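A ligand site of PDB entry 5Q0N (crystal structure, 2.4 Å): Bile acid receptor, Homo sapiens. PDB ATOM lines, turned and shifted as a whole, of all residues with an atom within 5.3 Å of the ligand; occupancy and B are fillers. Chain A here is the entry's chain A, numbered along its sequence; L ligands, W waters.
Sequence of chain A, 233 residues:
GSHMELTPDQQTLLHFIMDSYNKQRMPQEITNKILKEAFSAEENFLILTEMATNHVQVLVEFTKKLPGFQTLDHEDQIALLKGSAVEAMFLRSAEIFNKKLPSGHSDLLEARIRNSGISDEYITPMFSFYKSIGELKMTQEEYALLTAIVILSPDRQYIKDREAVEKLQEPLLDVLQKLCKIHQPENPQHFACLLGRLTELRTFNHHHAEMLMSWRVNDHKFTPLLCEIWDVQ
The side-chain hydroxyl of Tyr 130 sits close to the side-chain sulfur of Met 126 (3.7 Å).
The backbone carbonyl oxygen (O) of Arg 25 sits at hydrogen-bond distance from the guanidinium group (NH2) of Arg 92 (2.7 Å).
OE1 of Gln 24 lies within hydrogen-bond range of NH1 of Arg 92 (3.3 Å).
OG of Ser 93 lies within hydrogen-bond range of O of Met 89.
The side-chain sulfur (SD) of Met 51 lies within hydrogen-bond range of the guanidinium group (NH1) of Arg 25, 3.2 Å away.
OG of Ser 116 is in hydrogen-bond range of O of Ile 113, 2.7 Å away.
The indole nitrogen (NE1) of Trp 215 lies within hydrogen-bond range of the backbone carbonyl oxygen (O) of Ser 116 (3.2 Å).
Water W1 lies within hydrogen-bond range of O1 of the ligand, OD1 of Asn 54, O of Met 51 and NH1 of Arg 25.
N of Phe 97 sits close to F1 of the ligand (3.1 Å).
Merely in contact with the ligand: Ile 30 (3.6 Å), Ile 34 (3.6 Å), Asn 44 (3.6 Å), Ile 47 (3.9 Å), Leu 48 (3.6 Å), Met 51 (3.4 Å), Ala 52 (3.7 Å), His 55 (3.3 Å), Met 89 (3.6 Å), Phe 90 (3.7 Å), Ile 96 (3.3 Å), Leu 109 (3.9 Å), Ile 113 (3.7 Å), Ser 116 (3.8 Å), Met 126 (3.5 Å) and Met 211 (3.9 Å).
Hydrophobic or aromatic side chains that line the ligand: Ile 30, Ile 34, Ile 47, Leu 48, Met 51, His 55, Met 89, Phe 90, Ile 96, Phe 97, Leu 109, Ile 113, Met 126, Tyr 130 and Met 211.
20 residues have an atom within 4 Å of the ligand: Ile 30, Ile 34, Asn 44, Ile 47, Leu 48, Met 51, Ala 52, His 55, Met 89, Phe 90, Arg 92, Ser 93, Ile 96, Phe 97, Leu 109, Ile 113, Ser 116, Met 126, Tyr 130 and Met 211.
Along chain A the residues within 4 Å of the ligand span positions 30 to 211.
The side-chain hydroxyl of Tyr 130 is in hydrogen-bond range of a nitrogen (N2) of the ligand, at 2.8 Å.
The guanidinium group (NE) of Arg 92 is in salt-bridge range of an oxygen (O2) of the ligand.
OG of Ser 93 sits at hydrogen-bond distance from N3 of the ligand (3.1 Å).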
ATOM      1  N   GLN A  24     -24.922 -30.684   3.753  1.00  0.00           N
ATOM      2  CA  GLN A  24     -25.374 -30.290   5.093  1.00  0.00           C
ATOM      3  C   GLN A  24     -26.828 -29.835   5.116  1.00  0.00           C
ATOM      4  O   GLN A  24     -27.389 -29.521   4.062  1.00  0.00           O
ATOM      5  CB  GLN A  24     -24.511 -29.137   5.620  1.00  0.00           C
ATOM      6  CG  GLN A  24     -23.242 -29.583   6.296  1.00  0.00           C
ATOM      7  CD  GLN A  24     -22.487 -28.412   6.849  1.00  0.00           C
ATOM      8  OE1 GLN A  24     -22.225 -27.421   6.165  1.00  0.00           O
ATOM      9  NE2 GLN A  24     -22.105 -28.519   8.101  1.00  0.00           N
ATOM     10  N   ARG A  25     -27.419 -29.757   6.334  1.00  0.00           N
ATOM     11  CA  ARG A  25     -28.781 -29.273   6.573  1.00  0.00           C
ATOM     12  C   ARG A  25     -28.845 -27.798   6.112  1.00  0.00           C
ATOM     13  O   ARG A  25     -27.967 -27.018   6.470  1.00  0.00           O
ATOM     14  CB  ARG A  25     -29.163 -29.409   8.064  1.00  0.00           C
ATOM     15  CG  ARG A  25     -30.615 -29.050   8.373  1.00  0.00           C
ATOM     16  CD  ARG A  25     -31.035 -29.482   9.771  1.00  0.00           C
ATOM     17  NE  ARG A  25     -31.345 -30.924   9.836  1.00  0.00           N
ATOM     18  CZ  ARG A  25     -31.599 -31.593  10.947  1.00  0.00           C
ATOM     19  NH1 ARG A  25     -31.583 -30.983  12.127  1.00  0.00           N
ATOM     20  NH2 ARG A  25     -31.872 -32.899  10.905  1.00  0.00           N
ATOM     21  N   ILE A  30     -33.226 -24.127   9.361  1.00  0.00           N
ATOM     22  CA  ILE A  30     -32.808 -23.875  10.743  1.00  0.00           C
ATOM     23  C   ILE A  30     -33.343 -22.532  11.277  1.00  0.00           C
ATOM     24  O   ILE A  30     -33.968 -22.508  12.333  1.00  0.00           O
ATOM     25  CB  ILE A  30     -31.253 -24.015  10.853  1.00  0.00           C
ATOM     26  CG1 ILE A  30     -30.791 -25.430  10.419  1.00  0.00           C
ATOM     27  CG2 ILE A  30     -30.732 -23.626  12.248  1.00  0.00           C
ATOM     28  CD1 ILE A  30     -29.399 -25.533   9.815  1.00  0.00           C
ATOM     29  N   THR A  31     -33.077 -21.428  10.546  1.00  0.00           N
ATOM     30  CA  THR A  31     -33.495 -20.070  10.909  1.00  0.00           C
ATOM     31  C   THR A  31     -34.994 -19.874  10.819  1.00  0.00           C
ATOM     32  O   THR A  31     -35.545 -19.168  11.664  1.00  0.00           O
ATOM     33  CB  THR A  31     -32.744 -19.000  10.123  1.00  0.00           C
ATOM     34  OG1 THR A  31     -32.802 -19.291   8.723  1.00  0.00           O
ATOM     35  CG2 THR A  31     -31.319 -18.855  10.575  1.00  0.00           C
ATOM     36  N   ILE A  34     -36.522 -21.255  14.132  1.00  0.00           N
ATOM     37  CA  ILE A  34     -36.231 -20.380  15.284  1.00  0.00           C
ATOM     38  C   ILE A  34     -37.076 -19.090  15.201  1.00  0.00           C
ATOM     39  O   ILE A  34     -37.662 -18.689  16.218  1.00  0.00           O
ATOM     40  CB  ILE A  34     -34.698 -20.108  15.435  1.00  0.00           C
ATOM     41  CG1 ILE A  34     -33.902 -21.436  15.598  1.00  0.00           C
ATOM     42  CG2 ILE A  34     -34.405 -19.146  16.607  1.00  0.00           C
ATOM     43  CD1 ILE A  34     -32.337 -21.336  15.335  1.00  0.00           C
ATOM     44  N   ASN A  44     -36.229 -25.941  23.271  1.00  0.00           N
ATOM     45  CA  ASN A  44     -34.991 -25.516  22.625  1.00  0.00           C
ATOM     46  C   ASN A  44     -33.816 -26.466  22.918  1.00  0.00           C
ATOM     47  O   ASN A  44     -32.990 -26.691  22.034  1.00  0.00           O
ATOM     48  CB  ASN A  44     -34.637 -24.086  23.005  1.00  0.00           C
ATOM     49  CG  ASN A  44     -35.404 -23.037  22.221  1.00  0.00           C
ATOM     50  OD1 ASN A  44     -35.651 -23.160  21.012  1.00  0.00           O
ATOM     51  ND2 ASN A  44     -35.770 -21.944  22.880  1.00  0.00           N
ATOM     52  N   ILE A  47     -34.395 -29.353  20.607  1.00  0.00           N
ATOM     53  CA  ILE A  47     -34.059 -28.916  19.244  1.00  0.00           C
ATOM     54  C   ILE A  47     -32.517 -28.976  19.099  1.00  0.00           C
ATOM     55  O   ILE A  47     -32.024 -29.562  18.139  1.00  0.00           O
ATOM     56  CB  ILE A  47     -34.656 -27.495  18.916  1.00  0.00           C
ATOM     57  CG1 ILE A  47     -36.196 -27.539  18.801  1.00  0.00           C
ATOM     58  CG2 ILE A  47     -34.027 -26.876  17.651  1.00  0.00           C
ATOM     59  CD1 ILE A  47     -36.906 -26.217  19.050  1.00  0.00           C
ATOM     60  N   LEU A  48     -31.782 -28.430  20.095  1.00  0.00           N
ATOM     61  CA  LEU A  48     -30.316 -28.426  20.126  1.00  0.00           C
ATOM     62  C   LEU A  48     -29.753 -29.854  20.045  1.00  0.00           C
ATOM     63  O   LEU A  48     -28.890 -30.123  19.213  1.00  0.00           O
ATOM     64  CB  LEU A  48     -29.792 -27.698  21.388  1.00  0.00           C
ATOM     65  CG  LEU A  48     -28.267 -27.789  21.689  1.00  0.00           C
ATOM     66  CD1 LEU A  48     -27.427 -27.080  20.629  1.00  0.00           C
ATOM     67  CD2 LEU A  48     -27.947 -27.252  23.051  1.00  0.00           C
ATOM     68  N   MET A  51     -30.395 -31.346  16.504  1.00  0.00           N
ATOM     69  CA  MET A  51     -29.561 -30.636  15.532  1.00  0.00           C
ATOM     70  C   MET A  51     -28.098 -31.063  15.653  1.00  0.00           C
ATOM     71  O   MET A  51     -27.455 -31.312  14.634  1.00  0.00           O
ATOM     72  CB  MET A  51     -29.665 -29.109  15.738  1.00  0.00           C
ATOM     73  CG  MET A  51     -30.996 -28.508  15.332  1.00  0.00           C
ATOM     74  SD  MET A  51     -31.102 -28.211  13.573  1.00  0.00           S
ATOM     75  CE  MET A  51     -29.886 -27.026  13.374  1.00  0.00           C
ATOM     76  N   ALA A  52     -27.564 -31.102  16.899  1.00  0.00           N
ATOM     77  CA  ALA A  52     -26.180 -31.472  17.184  1.00  0.00           C
ATOM     78  C   ALA A  52     -25.873 -32.938  16.859  1.00  0.00           C
ATOM     79  O   ALA A  52     -24.766 -33.219  16.403  1.00  0.00           O
ATOM     80  CB  ALA A  52     -25.844 -31.157  18.616  1.00  0.00           C
ATOM     81  N   ASN A  54     -27.490 -34.819  14.484  1.00  0.00           N
ATOM     82  CA  ASN A  54     -27.459 -34.843  13.025  1.00  0.00           C
ATOM     83  C   ASN A  54     -26.160 -34.242  12.501  1.00  0.00           C
ATOM     84  O   ASN A  54     -25.568 -34.834  11.596  1.00  0.00           O
ATOM     85  CB  ASN A  54     -28.677 -34.135  12.409  1.00  0.00           C
ATOM     86  CG  ASN A  54     -28.633 -34.074  10.892  1.00  0.00           C
ATOM     87  OD1 ASN A  54     -28.497 -32.995  10.288  1.00  0.00           O
ATOM     88  ND2 ASN A  54     -28.677 -35.258  10.245  1.00  0.00           N
ATOM     89  N   HIS A  55     -25.714 -33.094  13.063  1.00  0.00           N
ATOM     90  CA  HIS A  55     -24.471 -32.421  12.679  1.00  0.00           C
ATOM     91  C   HIS A  55     -23.245 -33.361  12.788  1.00  0.00           C
ATOM     92  O   HIS A  55     -22.412 -33.365  11.880  1.00  0.00           O
ATOM     93  CB  HIS A  55     -24.282 -31.107  13.453  1.00  0.00           C
ATOM     94  CG  HIS A  55     -22.877 -30.579  13.404  1.00  0.00           C
ATOM     95  ND1 HIS A  55     -21.962 -30.988  14.374  1.00  0.00           N
ATOM     96  CD2 HIS A  55     -22.233 -29.827  12.498  1.00  0.00           C
ATOM     97  CE1 HIS A  55     -20.806 -30.447  14.037  1.00  0.00           C
ATOM     98  NE2 HIS A  55     -20.914 -29.759  12.898  1.00  0.00           N
ATOM     99  N   MET A  89     -19.346 -27.394  15.008  1.00  0.00           N
ATOM    100  CA  MET A  89     -20.730 -26.968  15.238  1.00  0.00           C
ATOM    101  C   MET A  89     -20.810 -25.442  15.490  1.00  0.00           C
ATOM    102  O   MET A  89     -21.681 -24.788  14.919  1.00  0.00           O
ATOM    103  CB  MET A  89     -21.377 -27.764  16.380  1.00  0.00           C
ATOM    104  CG  MET A  89     -22.735 -27.218  16.750  1.00  0.00           C
ATOM    105  SD  MET A  89     -23.216 -27.333  18.478  1.00  0.00           S
ATOM    106  CE  MET A  89     -21.690 -26.961  19.307  1.00  0.00           C
ATOM    107  N   PHE A  90     -19.895 -24.894  16.316  1.00  0.00           N
ATOM    108  CA  PHE A  90     -19.864 -23.449  16.548  1.00  0.00           C
ATOM    109  C   PHE A  90     -19.496 -22.671  15.301  1.00  0.00           C
ATOM    110  O   PHE A  90     -20.044 -21.580  15.104  1.00  0.00           O
ATOM    111  CB  PHE A  90     -18.990 -23.040  17.759  1.00  0.00           C
ATOM    112  CG  PHE A  90     -19.690 -23.307  19.066  1.00  0.00           C
ATOM    113  CD1 PHE A  90     -20.854 -22.616  19.403  1.00  0.00           C
ATOM    114  CD2 PHE A  90     -19.221 -24.276  19.946  1.00  0.00           C
ATOM    115  CE1 PHE A  90     -21.531 -22.874  20.576  1.00  0.00           C
ATOM    116  CE2 PHE A  90     -19.904 -24.537  21.132  1.00  0.00           C
ATOM    117  CZ  PHE A  90     -21.054 -23.831  21.447  1.00  0.00           C
ATOM    118  N   ARG A  92     -20.173 -23.677  12.198  1.00  0.00           N
ATOM    119  CA  ARG A  92     -21.391 -23.845  11.413  1.00  0.00           C
ATOM    120  C   ARG A  92     -22.506 -22.925  11.909  1.00  0.00           C
ATOM    121  O   ARG A  92     -23.195 -22.303  11.095  1.00  0.00           O
ATOM    122  CB  ARG A  92     -21.814 -25.328  11.405  1.00  0.00           C
ATOM    123  CG  ARG A  92     -23.089 -25.647  10.622  1.00  0.00           C
ATOM    124  CD  ARG A  92     -23.026 -25.204   9.180  1.00  0.00           C
ATOM    125  NE  ARG A  92     -24.263 -25.536   8.490  1.00  0.00           N
ATOM    126  CZ  ARG A  92     -24.528 -25.197   7.237  1.00  0.00           C
ATOM    127  NH1 ARG A  92     -23.647 -24.501   6.537  1.00  0.00           N
ATOM    128  NH2 ARG A  92     -25.676 -25.542   6.678  1.00  0.00           N
ATOM    129  N   SER A  93     -22.661 -22.785  13.239  1.00  0.00           N
ATOM    130  CA  SER A  93     -23.651 -21.903  13.881  1.00  0.00           C
ATOM    131  C   SER A  93     -23.315 -20.448  13.577  1.00  0.00           C
ATOM    132  O   SER A  93     -24.218 -19.656  13.348  1.00  0.00           O
ATOM    133  CB  SER A  93     -23.704 -22.125  15.383  1.00  0.00           C
ATOM    134  OG  SER A  93     -24.184 -23.428  15.670  1.00  0.00           O
ATOM    135  N   ALA A  94     -22.008 -20.122  13.528  1.00  0.00           N
ATOM    136  CA  ALA A  94     -21.497 -18.792  13.207  1.00  0.00           C
ATOM    137  C   ALA A  94     -21.839 -18.435  11.757  1.00  0.00           C
ATOM    138  O   ALA A  94     -22.248 -17.306  11.507  1.00  0.00           O
ATOM    139  CB  ALA A  94     -19.998 -18.741  13.432  1.00  0.00           C
ATOM    140  N   ILE A  96     -24.411 -19.669   9.829  1.00  0.00           N
ATOM    141  CA  ILE A  96     -25.867 -19.464   9.781  1.00  0.00           C
ATOM    142  C   ILE A  96     -26.255 -18.113  10.391  1.00  0.00           C
ATOM    143  O   ILE A  96     -27.007 -17.370   9.775  1.00  0.00           O
ATOM    144  CB  ILE A  96     -26.601 -20.678  10.388  1.00  0.00           C
ATOM    145  CG1 ILE A  96     -26.331 -21.943   9.555  1.00  0.00           C
ATOM    146  CG2 ILE A  96     -28.102 -20.423  10.483  1.00  0.00           C
ATOM    147  CD1 ILE A  96     -26.389 -23.164  10.273  1.00  0.00           C
ATOM    148  N   PHE A  97     -25.673 -17.746  11.560  1.00  0.00           N
ATOM    149  CA  PHE A  97     -25.937 -16.465  12.235  1.00  0.00           C
ATOM    150  C   PHE A  97     -25.620 -15.219  11.373  1.00  0.00           C
ATOM    151  O   PHE A  97     -26.272 -14.187  11.534  1.00  0.00           O
ATOM    152  CB  PHE A  97     -25.162 -16.410  13.572  1.00  0.00           C
ATOM    153  CG  PHE A  97     -25.469 -15.216  14.452  1.00  0.00           C
ATOM    154  CD1 PHE A  97     -26.574 -15.206  15.282  1.00  0.00           C
ATOM    155  CD2 PHE A  97     -24.642 -14.094  14.448  1.00  0.00           C
ATOM    156  CE1 PHE A  97     -26.854 -14.102  16.100  1.00  0.00           C
ATOM    157  CE2 PHE A  97     -24.924 -12.987  15.257  1.00  0.00           C
ATOM    158  CZ  PHE A  97     -26.018 -12.998  16.089  1.00  0.00           C
ATOM    159  N   LEU A 109     -33.534 -13.205  15.473  1.00  0.00           N
ATOM    160  CA  LEU A 109     -32.792 -14.462  15.562  1.00  0.00           C
ATOM    161  C   LEU A 109     -31.881 -14.438  16.788  1.00  0.00           C
ATOM    162  O   LEU A 109     -31.923 -15.362  17.593  1.00  0.00           O
ATOM    163  CB  LEU A 109     -32.000 -14.723  14.262  1.00  0.00           C
ATOM    164  CG  LEU A 109     -31.227 -16.062  14.162  1.00  0.00           C
ATOM    165  CD1 LEU A 109     -32.178 -17.242  13.942  1.00  0.00           C
ATOM    166  CD2 LEU A 109     -30.213 -16.005  13.054  1.00  0.00           C
ATOM    167  N   ILE A 113     -32.193 -16.695  20.250  1.00  0.00           N
ATOM    168  CA  ILE A 113     -31.044 -17.510  20.722  1.00  0.00           C
ATOM    169  C   ILE A 113     -30.649 -17.094  22.151  1.00  0.00           C
ATOM    170  O   ILE A 113     -30.393 -17.954  22.991  1.00  0.00           O
ATOM    171  CB  ILE A 113     -29.854 -17.534  19.715  1.00  0.00           C
ATOM    172  CG1 ILE A 113     -30.274 -18.131  18.358  1.00  0.00           C
ATOM    173  CG2 ILE A 113     -28.639 -18.301  20.276  1.00  0.00           C
ATOM    174  CD1 ILE A 113     -29.467 -17.722  17.224  1.00  0.00           C
ATOM    175  N   SER A 116     -32.988 -18.791  24.556  1.00  0.00           N
ATOM    176  CA  SER A 116     -33.155 -20.240  24.320  1.00  0.00           C
ATOM    177  C   SER A 116     -33.051 -21.138  25.571  1.00  0.00           C
ATOM    178  O   SER A 116     -33.539 -22.279  25.557  1.00  0.00           O
ATOM    179  CB  SER A 116     -32.188 -20.724  23.246  1.00  0.00           C
ATOM    180  OG  SER A 116     -30.839 -20.545  23.653  1.00  0.00           O
ATOM    181  N   ILE A 118     -29.779 -21.068  27.452  1.00  0.00           N
ATOM    182  CA  ILE A 118     -28.351 -20.922  27.806  1.00  0.00           C
ATOM    183  C   ILE A 118     -28.196 -19.856  28.905  1.00  0.00           C
ATOM    184  O   ILE A 118     -28.905 -18.837  28.867  1.00  0.00           O
ATOM    185  CB  ILE A 118     -27.431 -20.517  26.629  1.00  0.00           C
ATOM    186  CG1 ILE A 118     -28.158 -20.481  25.289  1.00  0.00           C
ATOM    187  CG2 ILE A 118     -26.189 -21.370  26.583  1.00  0.00           C
ATOM    188  CD1 ILE A 118     -27.769 -19.286  24.415  1.00  0.00           C
ATOM    189  N   MET A 126     -20.200 -16.372  23.261  1.00  0.00           N
ATOM    190  CA  MET A 126     -20.768 -16.955  22.046  1.00  0.00           C
ATOM    191  C   MET A 126     -21.084 -15.901  20.948  1.00  0.00           C
ATOM    192  O   MET A 126     -20.631 -16.087  19.819  1.00  0.00           O
ATOM    193  CB  MET A 126     -21.988 -17.802  22.381  1.00  0.00           C
ATOM    194  CG  MET A 126     -22.620 -18.470  21.186  1.00  0.00           C
ATOM    195  SD  MET A 126     -24.140 -19.346  21.560  1.00  0.00           S
ATOM    196  CE  MET A 126     -25.203 -18.025  21.955  1.00  0.00           C
ATOM    197  N   TYR A 130     -19.363 -15.064  17.158  1.00  0.00           N
ATOM    198  CA  TYR A 130     -20.217 -14.994  15.960  1.00  0.00           C
ATOM    199  C   TYR A 130     -20.033 -13.682  15.185  1.00  0.00           C
ATOM    200  O   TYR A 130     -19.927 -13.708  13.950  1.00  0.00           O
ATOM    201  CB  TYR A 130     -21.703 -15.168  16.311  1.00  0.00           C
ATOM    202  CG  TYR A 130     -22.111 -16.542  16.806  1.00  0.00           C
ATOM    203  CD1 TYR A 130     -21.260 -17.640  16.677  1.00  0.00           C
ATOM    204  CD2 TYR A 130     -23.375 -16.767  17.347  1.00  0.00           C
ATOM    205  CE1 TYR A 130     -21.634 -18.911  17.122  1.00  0.00           C
ATOM    206  CE2 TYR A 130     -23.764 -18.034  17.776  1.00  0.00           C
ATOM    207  CZ  TYR A 130     -22.890 -19.105  17.658  1.00  0.00           C
ATOM    208  OH  TYR A 130     -23.231 -20.335  18.146  1.00  0.00           O
ATOM    209  N   MET A 211     -21.697 -25.212  29.571  1.00  0.00           N
ATOM    210  CA  MET A 211     -22.622 -24.426  28.748  1.00  0.00           C
ATOM    211  C   MET A 211     -23.931 -25.200  28.560  1.00  0.00           C
ATOM    212  O   MET A 211     -25.022 -24.606  28.595  1.00  0.00           O
ATOM    213  CB  MET A 211     -21.945 -24.137  27.399  1.00  0.00           C
ATOM    214  CG  MET A 211     -22.593 -23.080  26.561  1.00  0.00           C
ATOM    215  SD  MET A 211     -21.487 -22.629  25.201  1.00  0.00           S
ATOM    216  CE  MET A 211     -22.574 -21.560  24.247  1.00  0.00           C
ATOM    217  N   LEU A 212     -23.817 -26.525  28.411  1.00  0.00           N
ATOM    218  CA  LEU A 212     -24.918 -27.465  28.240  1.00  0.00           C
ATOM    219  C   LEU A 212     -25.595 -27.836  29.547  1.00  0.00           C
ATOM    220  O   LEU A 212     -26.814 -27.972  29.562  1.00  0.00           O
ATOM    221  CB  LEU A 212     -24.452 -28.719  27.512  1.00  0.00           C
ATOM    222  CG  LEU A 212     -23.922 -28.507  26.114  1.00  0.00           C
ATOM    223  CD1 LEU A 212     -22.850 -29.495  25.786  1.00  0.00           C
ATOM    224  CD2 LEU A 212     -25.045 -28.520  25.092  1.00  0.00           C
ATOM    225  N   TRP A 215     -27.838 -24.931  31.086  1.00  0.00           N
ATOM    226  CA  TRP A 215     -29.070 -24.654  30.338  1.00  0.00           C
ATOM    227  C   TRP A 215     -30.249 -24.774  31.297  1.00  0.00           C
ATOM    228  O   TRP A 215     -30.301 -25.740  32.063  1.00  0.00           O
ATOM    229  CB  TRP A 215     -29.221 -25.657  29.188  1.00  0.00           C
ATOM    230  CG  TRP A 215     -30.115 -25.205  28.073  1.00  0.00           C
ATOM    231  CD1 TRP A 215     -31.473 -25.196  28.056  1.00  0.00           C
ATOM    232  CD2 TRP A 215     -29.703 -24.802  26.755  1.00  0.00           C
ATOM    233  NE1 TRP A 215     -31.941 -24.773  26.830  1.00  0.00           N
ATOM    234  CE2 TRP A 215     -30.872 -24.518  26.011  1.00  0.00           C
ATOM    235  CE3 TRP A 215     -28.448 -24.602  26.146  1.00  0.00           C
ATOM    236  CZ2 TRP A 215     -30.825 -24.062  24.695  1.00  0.00           C
ATOM    237  CZ3 TRP A 215     -28.408 -24.148  24.843  1.00  0.00           C
ATOM    238  CH2 TRP A 215     -29.588 -23.881  24.130  1.00  0.00           C
HETATM  239  N1  LIG L   1     -27.440 -22.598  17.584  1.00  0.00           N
HETATM  240  N2  LIG L   1     -25.921 -20.971  17.873  1.00  0.00           N
HETATM  241  C1  LIG L   1     -27.632 -21.704  16.540  1.00  0.00           C
HETATM  242  C2  LIG L   1     -26.694 -20.711  16.729  1.00  0.00           C
HETATM  243  C3  LIG L   1     -28.180 -24.801  16.607  1.00  0.00           C
HETATM  244  C4  LIG L   1     -28.223 -23.879  17.869  1.00  0.00           C
HETATM  245  C5  LIG L   1     -28.542 -21.719  15.499  1.00  0.00           C
HETATM  246  C6  LIG L   1     -26.642 -19.652  15.824  1.00  0.00           C
HETATM  247  C7  LIG L   1     -26.056 -27.909  11.204  1.00  0.00           C
HETATM  248  C8  LIG L   1     -27.543 -19.658  14.782  1.00  0.00           C
HETATM  249  C9  LIG L   1     -26.442 -26.898  14.844  1.00  0.00           C
HETATM  250  C10 LIG L   1     -26.863 -24.956  13.478  1.00  0.00           C
HETATM  251  C11 LIG L   1     -26.631 -25.729  12.346  1.00  0.00           C
HETATM  252  C12 LIG L   1     -26.056 -22.204  20.835  1.00  0.00           C
HETATM  253  O1  LIG L   1     -25.994 -29.184  11.424  1.00  0.00           O
HETATM  254  O2  LIG L   1     -25.923 -27.419  10.085  1.00  0.00           O
HETATM  255  C13 LIG L   1     -26.311 -27.077  12.442  1.00  0.00           C
HETATM  256  C14 LIG L   1     -26.771 -25.531  14.756  1.00  0.00           C
HETATM  257  N3  LIG L   1     -27.002 -24.777  15.926  1.00  0.00           N
HETATM  258  O3  LIG L   1     -29.147 -25.473  16.280  1.00  0.00           O
HETATM  259  C15 LIG L   1     -29.664 -23.556  18.327  1.00  0.00           C
HETATM  260  C16 LIG L   1     -30.273 -24.683  19.164  1.00  0.00           C
HETATM  261  C17 LIG L   1     -31.740 -24.388  19.526  1.00  0.00           C
HETATM  262  C18 LIG L   1     -31.882 -23.064  20.304  1.00  0.00           C
HETATM  263  C19 LIG L   1     -31.205 -21.899  19.563  1.00  0.00           C
HETATM  264  C20 LIG L   1     -29.732 -22.253  19.142  1.00  0.00           C
HETATM  265  C21 LIG L   1     -26.404 -22.102  18.352  1.00  0.00           C
HETATM  266  F1  LIG L   1     -27.520 -18.660  13.882  1.00  0.00           F
HETATM  267  C22 LIG L   1     -28.471 -20.679  14.627  1.00  0.00           C
HETATM  268  F2  LIG L   1     -29.325 -20.632  13.573  1.00  0.00           F
HETATM  269  C23 LIG L   1     -25.890 -22.770  19.569  1.00  0.00           C
HETATM  270  C24 LIG L   1     -25.578 -22.841  21.964  1.00  0.00           C
HETATM  271  C25 LIG L   1     -24.932 -24.065  21.833  1.00  0.00           C
HETATM  272 CL1  LIG L   1     -24.335 -24.884  23.247  1.00  0.00          CL
HETATM  273  C26 LIG L   1     -24.757 -24.647  20.593  1.00  0.00           C
HETATM  274  C27 LIG L   1     -25.235 -24.001  19.466  1.00  0.00           C
HETATM  275 CL2  LIG L   1     -26.318 -27.671  16.397  1.00  0.00          CL
HETATM  276  C28 LIG L   1     -26.222 -27.660  13.708  1.00  0.00           C
HETATM  277  O   HOH W   1     -28.251 -30.527  11.752  1.00  0.00           O
HETATM  278  O   HOH W   2     -25.027 -30.255   9.117  1.00  0.00           O
